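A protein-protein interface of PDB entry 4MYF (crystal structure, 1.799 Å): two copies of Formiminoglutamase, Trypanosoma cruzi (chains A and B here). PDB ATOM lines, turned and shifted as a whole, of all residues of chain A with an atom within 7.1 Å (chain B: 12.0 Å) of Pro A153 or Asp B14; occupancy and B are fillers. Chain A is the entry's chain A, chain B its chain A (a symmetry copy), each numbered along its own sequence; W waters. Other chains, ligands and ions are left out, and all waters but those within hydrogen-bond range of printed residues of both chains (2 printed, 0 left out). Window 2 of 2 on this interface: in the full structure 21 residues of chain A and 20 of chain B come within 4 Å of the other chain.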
ATOM      1  N   VAL A 151      29.576  16.149 -17.679  1.00  0.00           N
ATOM      2  CA  VAL A 151      28.801  14.982 -18.125  1.00  0.00           C
ATOM      3  C   VAL A 151      27.384  14.928 -17.520  1.00  0.00           C
ATOM      4  O   VAL A 151      26.615  13.991 -17.756  1.00  0.00           O
ATOM      5  CB  VAL A 151      29.616  13.669 -17.886  1.00  0.00           C
ATOM      6  CG1 VAL A 151      28.764  12.550 -17.320  1.00  0.00           C
ATOM      7  CG2 VAL A 151      30.329  13.245 -19.163  1.00  0.00           C
ATOM      8  N   ARG A 152      27.029  15.962 -16.766  1.00  0.00           N
ATOM      9  CA  ARG A 152      25.697  16.051 -16.180  1.00  0.00           C
ATOM     10  C   ARG A 152      24.611  15.925 -17.249  1.00  0.00           C
ATOM     11  O   ARG A 152      24.774  16.408 -18.373  1.00  0.00           O
ATOM     12  CB  ARG A 152      25.537  17.364 -15.400  1.00  0.00           C
ATOM     13  CG  ARG A 152      24.139  17.607 -14.838  1.00  0.00           C
ATOM     14  CD  ARG A 152      24.160  18.580 -13.660  1.00  0.00           C
ATOM     15  NE  ARG A 152      24.890  18.041 -12.514  1.00  0.00           N
ATOM     16  CZ  ARG A 152      24.915  18.604 -11.308  1.00  0.00           C
ATOM     17  NH1 ARG A 152      24.243  19.724 -11.080  1.00  0.00           N
ATOM     18  NH2 ARG A 152      25.608  18.041 -10.326  1.00  0.00           N
ATOM     19  N   PRO A 153      23.504  15.251 -16.903  1.00  0.00           N
ATOM     20  CA  PRO A 153      22.339  15.130 -17.790  1.00  0.00           C
ATOM     21  C   PRO A 153      21.855  16.488 -18.298  1.00  0.00           C
ATOM     22  O   PRO A 153      21.164  16.531 -19.319  1.00  0.00           O
ATOM     23  CB  PRO A 153      21.281  14.497 -16.883  1.00  0.00           C
ATOM     24  CG  PRO A 153      22.070  13.704 -15.891  1.00  0.00           C
ATOM     25  CD  PRO A 153      23.344  14.475 -15.659  1.00  0.00           C
ATOM     26  N   GLY A 163      22.491  20.204 -22.581  1.00  0.00           N
ATOM     27  CA  GLY A 163      23.210  19.557 -21.497  1.00  0.00           C
ATOM     28  C   GLY A 163      24.716  19.729 -21.616  1.00  0.00           C
ATOM     29  O   GLY A 163      25.198  20.440 -22.494  1.00  0.00           O
ATOM     30  N   THR A 164      25.459  19.079 -20.728  1.00  0.00           N
ATOM     31  CA  THR A 164      26.909  19.158 -20.767  1.00  0.00           C
ATOM     32  C   THR A 164      27.432  18.597 -22.079  1.00  0.00           C
ATOM     33  O   THR A 164      26.908  17.605 -22.599  1.00  0.00           O
ATOM     34  CB  THR A 164      27.561  18.390 -19.613  1.00  0.00           C
ATOM     35  OG1 THR A 164      27.064  17.047 -19.599  1.00  0.00           O
ATOM     36  CG2 THR A 164      27.268  19.064 -18.290  1.00  0.00           C
ATOM     37  N   ARG A 167      28.558  14.750 -22.411  1.00  0.00           N
ATOM     38  CA  ARG A 167      27.469  13.783 -22.373  1.00  0.00           C
ATOM     39  C   ARG A 167      26.832  13.715 -23.754  1.00  0.00           C
ATOM     40  O   ARG A 167      26.474  12.643 -24.232  1.00  0.00           O
ATOM     41  CB  ARG A 167      26.419  14.137 -21.323  1.00  0.00           C
ATOM     42  CG  ARG A 167      25.374  13.044 -21.170  1.00  0.00           C
ATOM     43  CD  ARG A 167      24.396  13.320 -20.051  1.00  0.00           C
ATOM     44  NE  ARG A 167      23.643  12.113 -19.717  1.00  0.00           N
ATOM     45  CZ  ARG A 167      23.838  11.390 -18.620  1.00  0.00           C
ATOM     46  NH1 ARG A 167      24.751  11.762 -17.735  1.00  0.00           N
ATOM     47  NH2 ARG A 167      23.110  10.304 -18.400  1.00  0.00           N
ATOM     48  N   GLU A 171      26.882  10.298 -26.119  1.00  0.00           N
ATOM     49  CA  GLU A 171      25.606   9.770 -26.588  1.00  0.00           C
ATOM     50  C   GLU A 171      25.535   9.639 -28.113  1.00  0.00           C
ATOM     51  O   GLU A 171      24.544   9.152 -28.653  1.00  0.00           O
ATOM     52  CB  GLU A 171      24.442  10.596 -26.030  1.00  0.00           C
ATOM     53  CG  GLU A 171      24.065  10.200 -24.602  1.00  0.00           C
ATOM     54  CD  GLU A 171      23.034  11.120 -23.971  1.00  0.00           C
ATOM     55  OE1 GLU A 171      22.640  12.116 -24.614  1.00  0.00           O
ATOM     56  OE2 GLU A 171      22.620  10.847 -22.821  1.00  0.00           O
ATOM     57  N   CYS A 190      34.021  15.733  -8.723  1.00  0.00           N
ATOM     58  CA  CYS A 190      33.401  14.811  -9.657  1.00  0.00           C
ATOM     59  C   CYS A 190      32.511  13.788  -8.937  1.00  0.00           C
ATOM     60  O   CYS A 190      32.947  13.051  -8.056  1.00  0.00           O
ATOM     61  CB  CYS A 190      34.469  14.179 -10.568  1.00  0.00           C
ATOM     62  SG  CYS A 190      35.437  15.411 -11.565  1.00  0.00           S
ATOM     63  N   GLY A 191      31.232  13.784  -9.304  1.00  0.00           N
ATOM     64  CA  GLY A 191      30.293  12.867  -8.677  1.00  0.00           C
ATOM     65  C   GLY A 191      30.610  11.425  -9.042  1.00  0.00           C
ATOM     66  O   GLY A 191      31.141  11.167 -10.119  1.00  0.00           O
ATOM     67  N   ALA A 192      30.301  10.489  -8.146  1.00  0.00           N
ATOM     68  CA  ALA A 192      30.421   9.069  -8.461  1.00  0.00           C
ATOM     69  C   ALA A 192      29.577   8.675  -9.673  1.00  0.00           C
ATOM     70  O   ALA A 192      30.011   7.870 -10.498  1.00  0.00           O
ATOM     71  CB  ALA A 192      30.055   8.221  -7.263  1.00  0.00           C
ATOM     72  N   LEU A 193      28.368   9.225  -9.779  1.00  0.00           N
ATOM     73  CA  LEU A 193      27.505   8.924 -10.927  1.00  0.00           C
ATOM     74  C   LEU A 193      28.124   9.390 -12.248  1.00  0.00           C
ATOM     75  O   LEU A 193      27.950   8.752 -13.289  1.00  0.00           O
ATOM     76  CB  LEU A 193      26.123   9.553 -10.747  1.00  0.00           C
ATOM     77  CG  LEU A 193      25.278   8.953  -9.616  1.00  0.00           C
ATOM     78  CD1 LEU A 193      23.972   9.710  -9.454  1.00  0.00           C
ATOM     79  CD2 LEU A 193      25.007   7.485  -9.872  1.00  0.00           C
ATOM     80  N   HIS A 194      28.845  10.509 -12.198  1.00  0.00           N
ATOM     81  CA  HIS A 194      29.502  11.062 -13.387  1.00  0.00           C
ATOM     82  C   HIS A 194      30.689  10.215 -13.845  1.00  0.00           C
ATOM     83  O   HIS A 194      30.814   9.901 -15.025  1.00  0.00           O
ATOM     84  CB  HIS A 194      29.929  12.511 -13.139  1.00  0.00           C
ATOM     85  CG  HIS A 194      28.781  13.472 -13.099  1.00  0.00           C
ATOM     86  ND1 HIS A 194      28.231  13.931 -11.920  1.00  0.00           N
ATOM     87  CD2 HIS A 194      28.063  14.045 -14.094  1.00  0.00           C
ATOM     88  CE1 HIS A 194      27.233  14.752 -12.190  1.00  0.00           C
ATOM     89  NE2 HIS A 194      27.108  14.839 -13.501  1.00  0.00           N
ATOM     90  N   THR B  13      20.711  15.339  -5.606  1.00  0.00           N
ATOM     91  CA  THR B  13      21.094  15.383  -7.012  1.00  0.00           C
ATOM     92  C   THR B  13      22.065  14.257  -7.357  1.00  0.00           C
ATOM     93  O   THR B  13      22.154  13.255  -6.642  1.00  0.00           O
ATOM     94  CB  THR B  13      21.734  16.737  -7.391  1.00  0.00           C
ATOM     95  OG1 THR B  13      22.885  16.973  -6.566  1.00  0.00           O
ATOM     96  CG2 THR B  13      20.737  17.876  -7.213  1.00  0.00           C
ATOM     97  N   ASP B  14      22.799  14.432  -8.451  1.00  0.00           N
ATOM     98  CA  ASP B  14      23.700  13.389  -8.924  1.00  0.00           C
ATOM     99  C   ASP B  14      25.157  13.604  -8.497  1.00  0.00           C
ATOM    100  O   ASP B  14      26.071  12.964  -9.027  1.00  0.00           O
ATOM    101  CB  ASP B  14      23.580  13.215 -10.446  1.00  0.00           C
ATOM    102  CG  ASP B  14      23.786  14.515 -11.205  1.00  0.00           C
ATOM    103  OD1 ASP B  14      23.959  15.569 -10.553  1.00  0.00           O
ATOM    104  OD2 ASP B  14      23.779  14.477 -12.460  1.00  0.00           O
ATOM    105  N   ASP B  15      25.365  14.489  -7.525  1.00  0.00           N
ATOM    106  CA  ASP B  15      26.704  14.734  -6.983  1.00  0.00           C
ATOM    107  C   ASP B  15      26.631  15.259  -5.543  1.00  0.00           C
ATOM    108  O   ASP B  15      26.852  16.445  -5.300  1.00  0.00           O
ATOM    109  CB  ASP B  15      27.472  15.715  -7.886  1.00  0.00           C
ATOM    110  CG  ASP B  15      28.939  15.875  -7.486  1.00  0.00           C
ATOM    111  OD1 ASP B  15      29.440  15.101  -6.636  1.00  0.00           O
ATOM    112  OD2 ASP B  15      29.602  16.783  -8.039  1.00  0.00           O
ATOM    113  N   PRO B  16      26.314  14.369  -4.584  1.00  0.00           N
ATOM    114  CA  PRO B  16      26.200  14.732  -3.167  1.00  0.00           C
ATOM    115  C   PRO B  16      27.516  15.291  -2.647  1.00  0.00           C
ATOM    116  O   PRO B  16      28.573  14.734  -2.940  1.00  0.00           O
ATOM    117  CB  PRO B  16      25.908  13.393  -2.481  1.00  0.00           C
ATOM    118  CG  PRO B  16      25.351  12.523  -3.555  1.00  0.00           C
ATOM    119  CD  PRO B  16      26.057  12.936  -4.808  1.00  0.00           C
ATOM    120  N   ARG B  17      27.440  16.380  -1.885  1.00  0.00           N
ATOM    121  CA  ARG B  17      28.632  17.049  -1.378  1.00  0.00           C
ATOM    122  C   ARG B  17      28.564  17.200   0.130  1.00  0.00           C
ATOM    123  O   ARG B  17      27.671  16.652   0.760  1.00  0.00           O
ATOM    124  CB  ARG B  17      28.827  18.392  -2.088  1.00  0.00           C
ATOM    125  CG  ARG B  17      29.016  18.196  -3.580  1.00  0.00           C
ATOM    126  CD  ARG B  17      29.447  19.441  -4.313  1.00  0.00           C
ATOM    127  NE  ARG B  17      30.043  19.087  -5.599  1.00  0.00           N
ATOM    128  CZ  ARG B  17      30.591  19.958  -6.441  1.00  0.00           C
ATOM    129  NH1 ARG B  17      30.616  21.250  -6.137  1.00  0.00           N
ATOM    130  NH2 ARG B  17      31.116  19.537  -7.584  1.00  0.00           N
ATOM    131  N   LEU B  18      29.524  17.914   0.712  1.00  0.00           N
ATOM    132  CA  LEU B  18      29.598  18.045   2.163  1.00  0.00           C
ATOM    133  C   LEU B  18      28.248  18.397   2.789  1.00  0.00           C
ATOM    134  O   LEU B  18      27.900  17.887   3.855  1.00  0.00           O
ATOM    135  CB  LEU B  18      30.652  19.095   2.563  1.00  0.00           C
ATOM    136  CG  LEU B  18      32.126  18.659   2.486  1.00  0.00           C
ATOM    137  CD1 LEU B  18      33.066  19.836   2.792  1.00  0.00           C
ATOM    138  CD2 LEU B  18      32.400  17.484   3.431  1.00  0.00           C
ATOM    139  N   SER B  20      25.415  17.490   2.129  1.00  0.00           N
ATOM    140  CA  SER B  20      24.593  16.298   2.306  1.00  0.00           C
ATOM    141  C   SER B  20      24.917  15.517   3.584  1.00  0.00           C
ATOM    142  O   SER B  20      24.139  14.660   3.997  1.00  0.00           O
ATOM    143  CB  SER B  20      24.742  15.373   1.101  1.00  0.00           C
ATOM    144  OG  SER B  20      25.956  14.651   1.193  1.00  0.00           O
ATOM    145  N   ARG B  65      28.504  24.301  -0.625  1.00  0.00           N
ATOM    146  CA  ARG B  65      28.645  24.161  -2.065  1.00  0.00           C
ATOM    147  C   ARG B  65      29.673  23.140  -2.550  1.00  0.00           C
ATOM    148  O   ARG B  65      29.573  22.663  -3.679  1.00  0.00           O
ATOM    149  CB  ARG B  65      28.965  25.523  -2.683  1.00  0.00           C
ATOM    150  CG  ARG B  65      27.814  26.515  -2.583  1.00  0.00           C
ATOM    151  CD  ARG B  65      28.247  27.957  -2.866  1.00  0.00           C
ATOM    152  NE  ARG B  65      27.071  28.809  -3.047  1.00  0.00           N
ATOM    153  CZ  ARG B  65      26.356  29.333  -2.052  1.00  0.00           C
ATOM    154  NH1 ARG B  65      26.697  29.118  -0.782  1.00  0.00           N
ATOM    155  NH2 ARG B  65      25.294  30.080  -2.329  1.00  0.00           N
ATOM    156  N   LEU B  66      30.650  22.804  -1.714  1.00  0.00           N
ATOM    157  CA  LEU B  66      31.822  22.080  -2.212  1.00  0.00           C
ATOM    158  C   LEU B  66      31.978  20.675  -1.651  1.00  0.00           C
ATOM    159  O   LEU B  66      31.413  20.348  -0.618  1.00  0.00           O
ATOM    160  CB  LEU B  66      33.099  22.870  -1.908  1.00  0.00           C
ATOM    161  CG  LEU B  66      33.181  24.316  -2.395  1.00  0.00           C
ATOM    162  CD1 LEU B  66      34.500  24.955  -1.959  1.00  0.00           C
ATOM    163  CD2 LEU B  66      33.021  24.382  -3.913  1.00  0.00           C
ATOM    164  N   GLY B  67      32.749  19.854  -2.358  1.00  0.00           N
ATOM    165  CA  GLY B  67      33.294  18.630  -1.796  1.00  0.00           C
ATOM    166  C   GLY B  67      32.503  17.361  -2.044  1.00  0.00           C
ATOM    167  O   GLY B  67      31.629  17.016  -1.253  1.00  0.00           O
ATOM    168  N   SER B  68      32.843  16.649  -3.115  1.00  0.00           N
ATOM    169  CA  SER B  68      32.200  15.368  -3.431  1.00  0.00           C
ATOM    170  C   SER B  68      32.398  14.353  -2.315  1.00  0.00           C
ATOM    171  O   SER B  68      33.527  13.996  -1.984  1.00  0.00           O
ATOM    172  CB  SER B  68      32.734  14.802  -4.750  1.00  0.00           C
ATOM    173  OG  SER B  68      32.440  15.660  -5.835  1.00  0.00           O
ATOM    174  N   VAL B  69      31.294  13.866  -1.745  1.00  0.00           N
ATOM    175  CA  VAL B  69      31.381  12.981  -0.589  1.00  0.00           C
ATOM    176  C   VAL B  69      32.012  11.630  -0.951  1.00  0.00           C
ATOM    177  O   VAL B  69      32.723  11.025  -0.147  1.00  0.00           O
ATOM    178  CB  VAL B  69      30.000  12.771   0.078  1.00  0.00           C
ATOM    179  CG1 VAL B  69      29.467  14.090   0.619  1.00  0.00           C
ATOM    180  CG2 VAL B  69      29.016  12.147  -0.908  1.00  0.00           C
ATOM    181  N   ASN B  70      31.753  11.157  -2.161  1.00  0.00           N
ATOM    182  CA  ASN B  70      32.480   9.997  -2.646  1.00  0.00           C
ATOM    183  C   ASN B  70      33.528  10.453  -3.649  1.00  0.00           C
ATOM    184  O   ASN B  70      33.205  10.832  -4.777  1.00  0.00           O
ATOM    185  CB  ASN B  70      31.536   8.955  -3.256  1.00  0.00           C
ATOM    186  CG  ASN B  70      32.209   7.608  -3.453  1.00  0.00           C
ATOM    187  OD1 ASN B  70      33.419   7.468  -3.257  1.00  0.00           O
ATOM    188  ND2 ASN B  70      31.427   6.609  -3.848  1.00  0.00           N
ATOM    189  N   ASN B  71      34.781  10.441  -3.212  1.00  0.00           N
ATOM    190  CA  ASN B  71      35.898  10.913  -4.014  1.00  0.00           C
ATOM    191  C   ASN B  71      36.560   9.736  -4.733  1.00  0.00           C
ATOM    192  O   ASN B  71      37.225   8.913  -4.105  1.00  0.00           O
ATOM    193  CB  ASN B  71      36.913  11.624  -3.099  1.00  0.00           C
ATOM    194  CG  ASN B  71      38.080  12.228  -3.867  1.00  0.00           C
ATOM    195  OD1 ASN B  71      38.639  11.599  -4.765  1.00  0.00           O
ATOM    196  ND2 ASN B  71      38.465  13.455  -3.500  1.00  0.00           N
ATOM    197  N   LEU B  72      36.385   9.658  -6.049  1.00  0.00           N
ATOM    198  CA  LEU B  72      36.904   8.521  -6.807  1.00  0.00           C
ATOM    199  C   LEU B  72      38.383   8.656  -7.172  1.00  0.00           C
ATOM    200  O   LEU B  72      39.007   7.706  -7.664  1.00  0.00           O
ATOM    201  CB  LEU B  72      36.051   8.277  -8.051  1.00  0.00           C
ATOM    202  CG  LEU B  72      34.701   7.631  -7.715  1.00  0.00           C
ATOM    203  CD1 LEU B  72      33.722   7.797  -8.850  1.00  0.00           C
ATOM    204  CD2 LEU B  72      34.899   6.163  -7.371  1.00  0.00           C
ATOM    205  N   ASP B  77      34.948   7.097   0.374  1.00  0.00           N
ATOM    206  CA  ASP B  77      33.545   7.472   0.413  1.00  0.00           C
ATOM    207  C   ASP B  77      33.209   7.953   1.824  1.00  0.00           C
ATOM    208  O   ASP B  77      33.236   7.169   2.765  1.00  0.00           O
ATOM    209  CB  ASP B  77      32.687   6.260   0.043  1.00  0.00           C
ATOM    210  CG  ASP B  77      31.200   6.575   0.006  1.00  0.00           C
ATOM    211  OD1 ASP B  77      30.806   7.716   0.323  1.00  0.00           O
ATOM    212  OD2 ASP B  77      30.421   5.668  -0.347  1.00  0.00           O
ATOM    213  N   SER B  79      30.339   9.059   2.841  1.00  0.00           N
ATOM    214  CA  SER B  79      28.882   8.999   2.991  1.00  0.00           C
ATOM    215  C   SER B  79      28.367   8.672   4.391  1.00  0.00           C
ATOM    216  O   SER B  79      27.304   9.155   4.787  1.00  0.00           O
ATOM    217  CB  SER B  79      28.282   8.006   1.983  1.00  0.00           C
ATOM    218  OG  SER B  79      28.319   8.543   0.676  1.00  0.00           O
HETATM  219  O   HOH W   1      27.473  11.239  -7.672  1.00  0.00           O
HETATM  220  O   HOH W   2      34.994  11.861  -7.045  1.00  0.00           O
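Among the printed residues, merely in contact across the chains: Arg A152 with Asp B15, Pro A153 with Asp B14, Cys A190 with Asn B70, Ala A192 with Leu B72, Leu A193 with Asp B14 and His A194 with Asp B14.
No residue of chain B comes within 4 Å of Val A151.
Arg A152 touches two residues of chain B.
Pro A153 touches one residue of chain B.
Gly A163 touches none of the printed residues of chain B.
No residue of chain B comes within 4 Å of Thr A164.
Of the printed residues of chain B, Ala A192 touches Leu B72.
Leu A193 touches just one residue of chain B: Asp B14 (3.7 Å).
Of chain A, only Arg A152, Pro A153, Leu A193 and His A194 come within 4 Å of Asp B14.
Printed residues of chain A within 4 Å of Asp B15: Arg A152 and Gly A191.
Of the printed residues of chain A, Asn B70 touches Cys A190 (3.97 Å).
The nearest printed residue of chain B that does not touch Pro A153 is Asp B15 (8.4 Å).
The backbone carbonyl oxygen (O) of Arg A152 sits at hydrogen-bond distance from the side-chain hydroxyl (OG1) of Thr A164.
A ring nitrogen (NE2) of His A194 lies close to the backbone NH (N) of Arg A152.
The side-chain carboxylate (OD2) of Asp B15 lies within salt-bridge range of the guanidinium group (NH2) of Arg B17 (3.2 Å).
OD1 of Asp B15 lies within hydrogen-bond range of OG of Ser B68, at 3.2 Å.
Water W2 lies within hydrogen-bond range of the backbone carbonyl oxygen (O) of Cys A190, the backbone NH (N) of Leu B72 and the backbone carbonyl oxygen (O) of Asn B70.
Water W1 lies within hydrogen-bond range of O of Asp B14 (2.6 Å), N of Ala A192 (3.0 Å) and N of Leu A193 (3.0 Å).
OD1 of Asp B14 lies within salt-bridge range of NH2 of Arg A152.
N of Cys A190 sits at hydrogen-bond distance from OG of Ser B68.
The backbone NH of Gly A191 sits close to the side-chain carboxylate of Asp B15.
No position is printed for both chains.
Printed residues of chain B that touch a printed residue of chain A: Asp B14, Asp B15, Ser B68, Asn B70 and Leu B72.
Hydrophobic or aromatic side chains of chain B within 4 Å of the printed part of chain A: Leu B72.
Along chain A the printed residues that touch a printed residue of chain B span positions 152 to 194.
Among the printed residues, 9 pairs touch across the chains.
Among the printed residues, Asp or Glu carboxylates within 4 Å of a Lys or Arg side-chain nitrogen of the other chain: Arg A152 with Asp B14 (3.0 Å).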
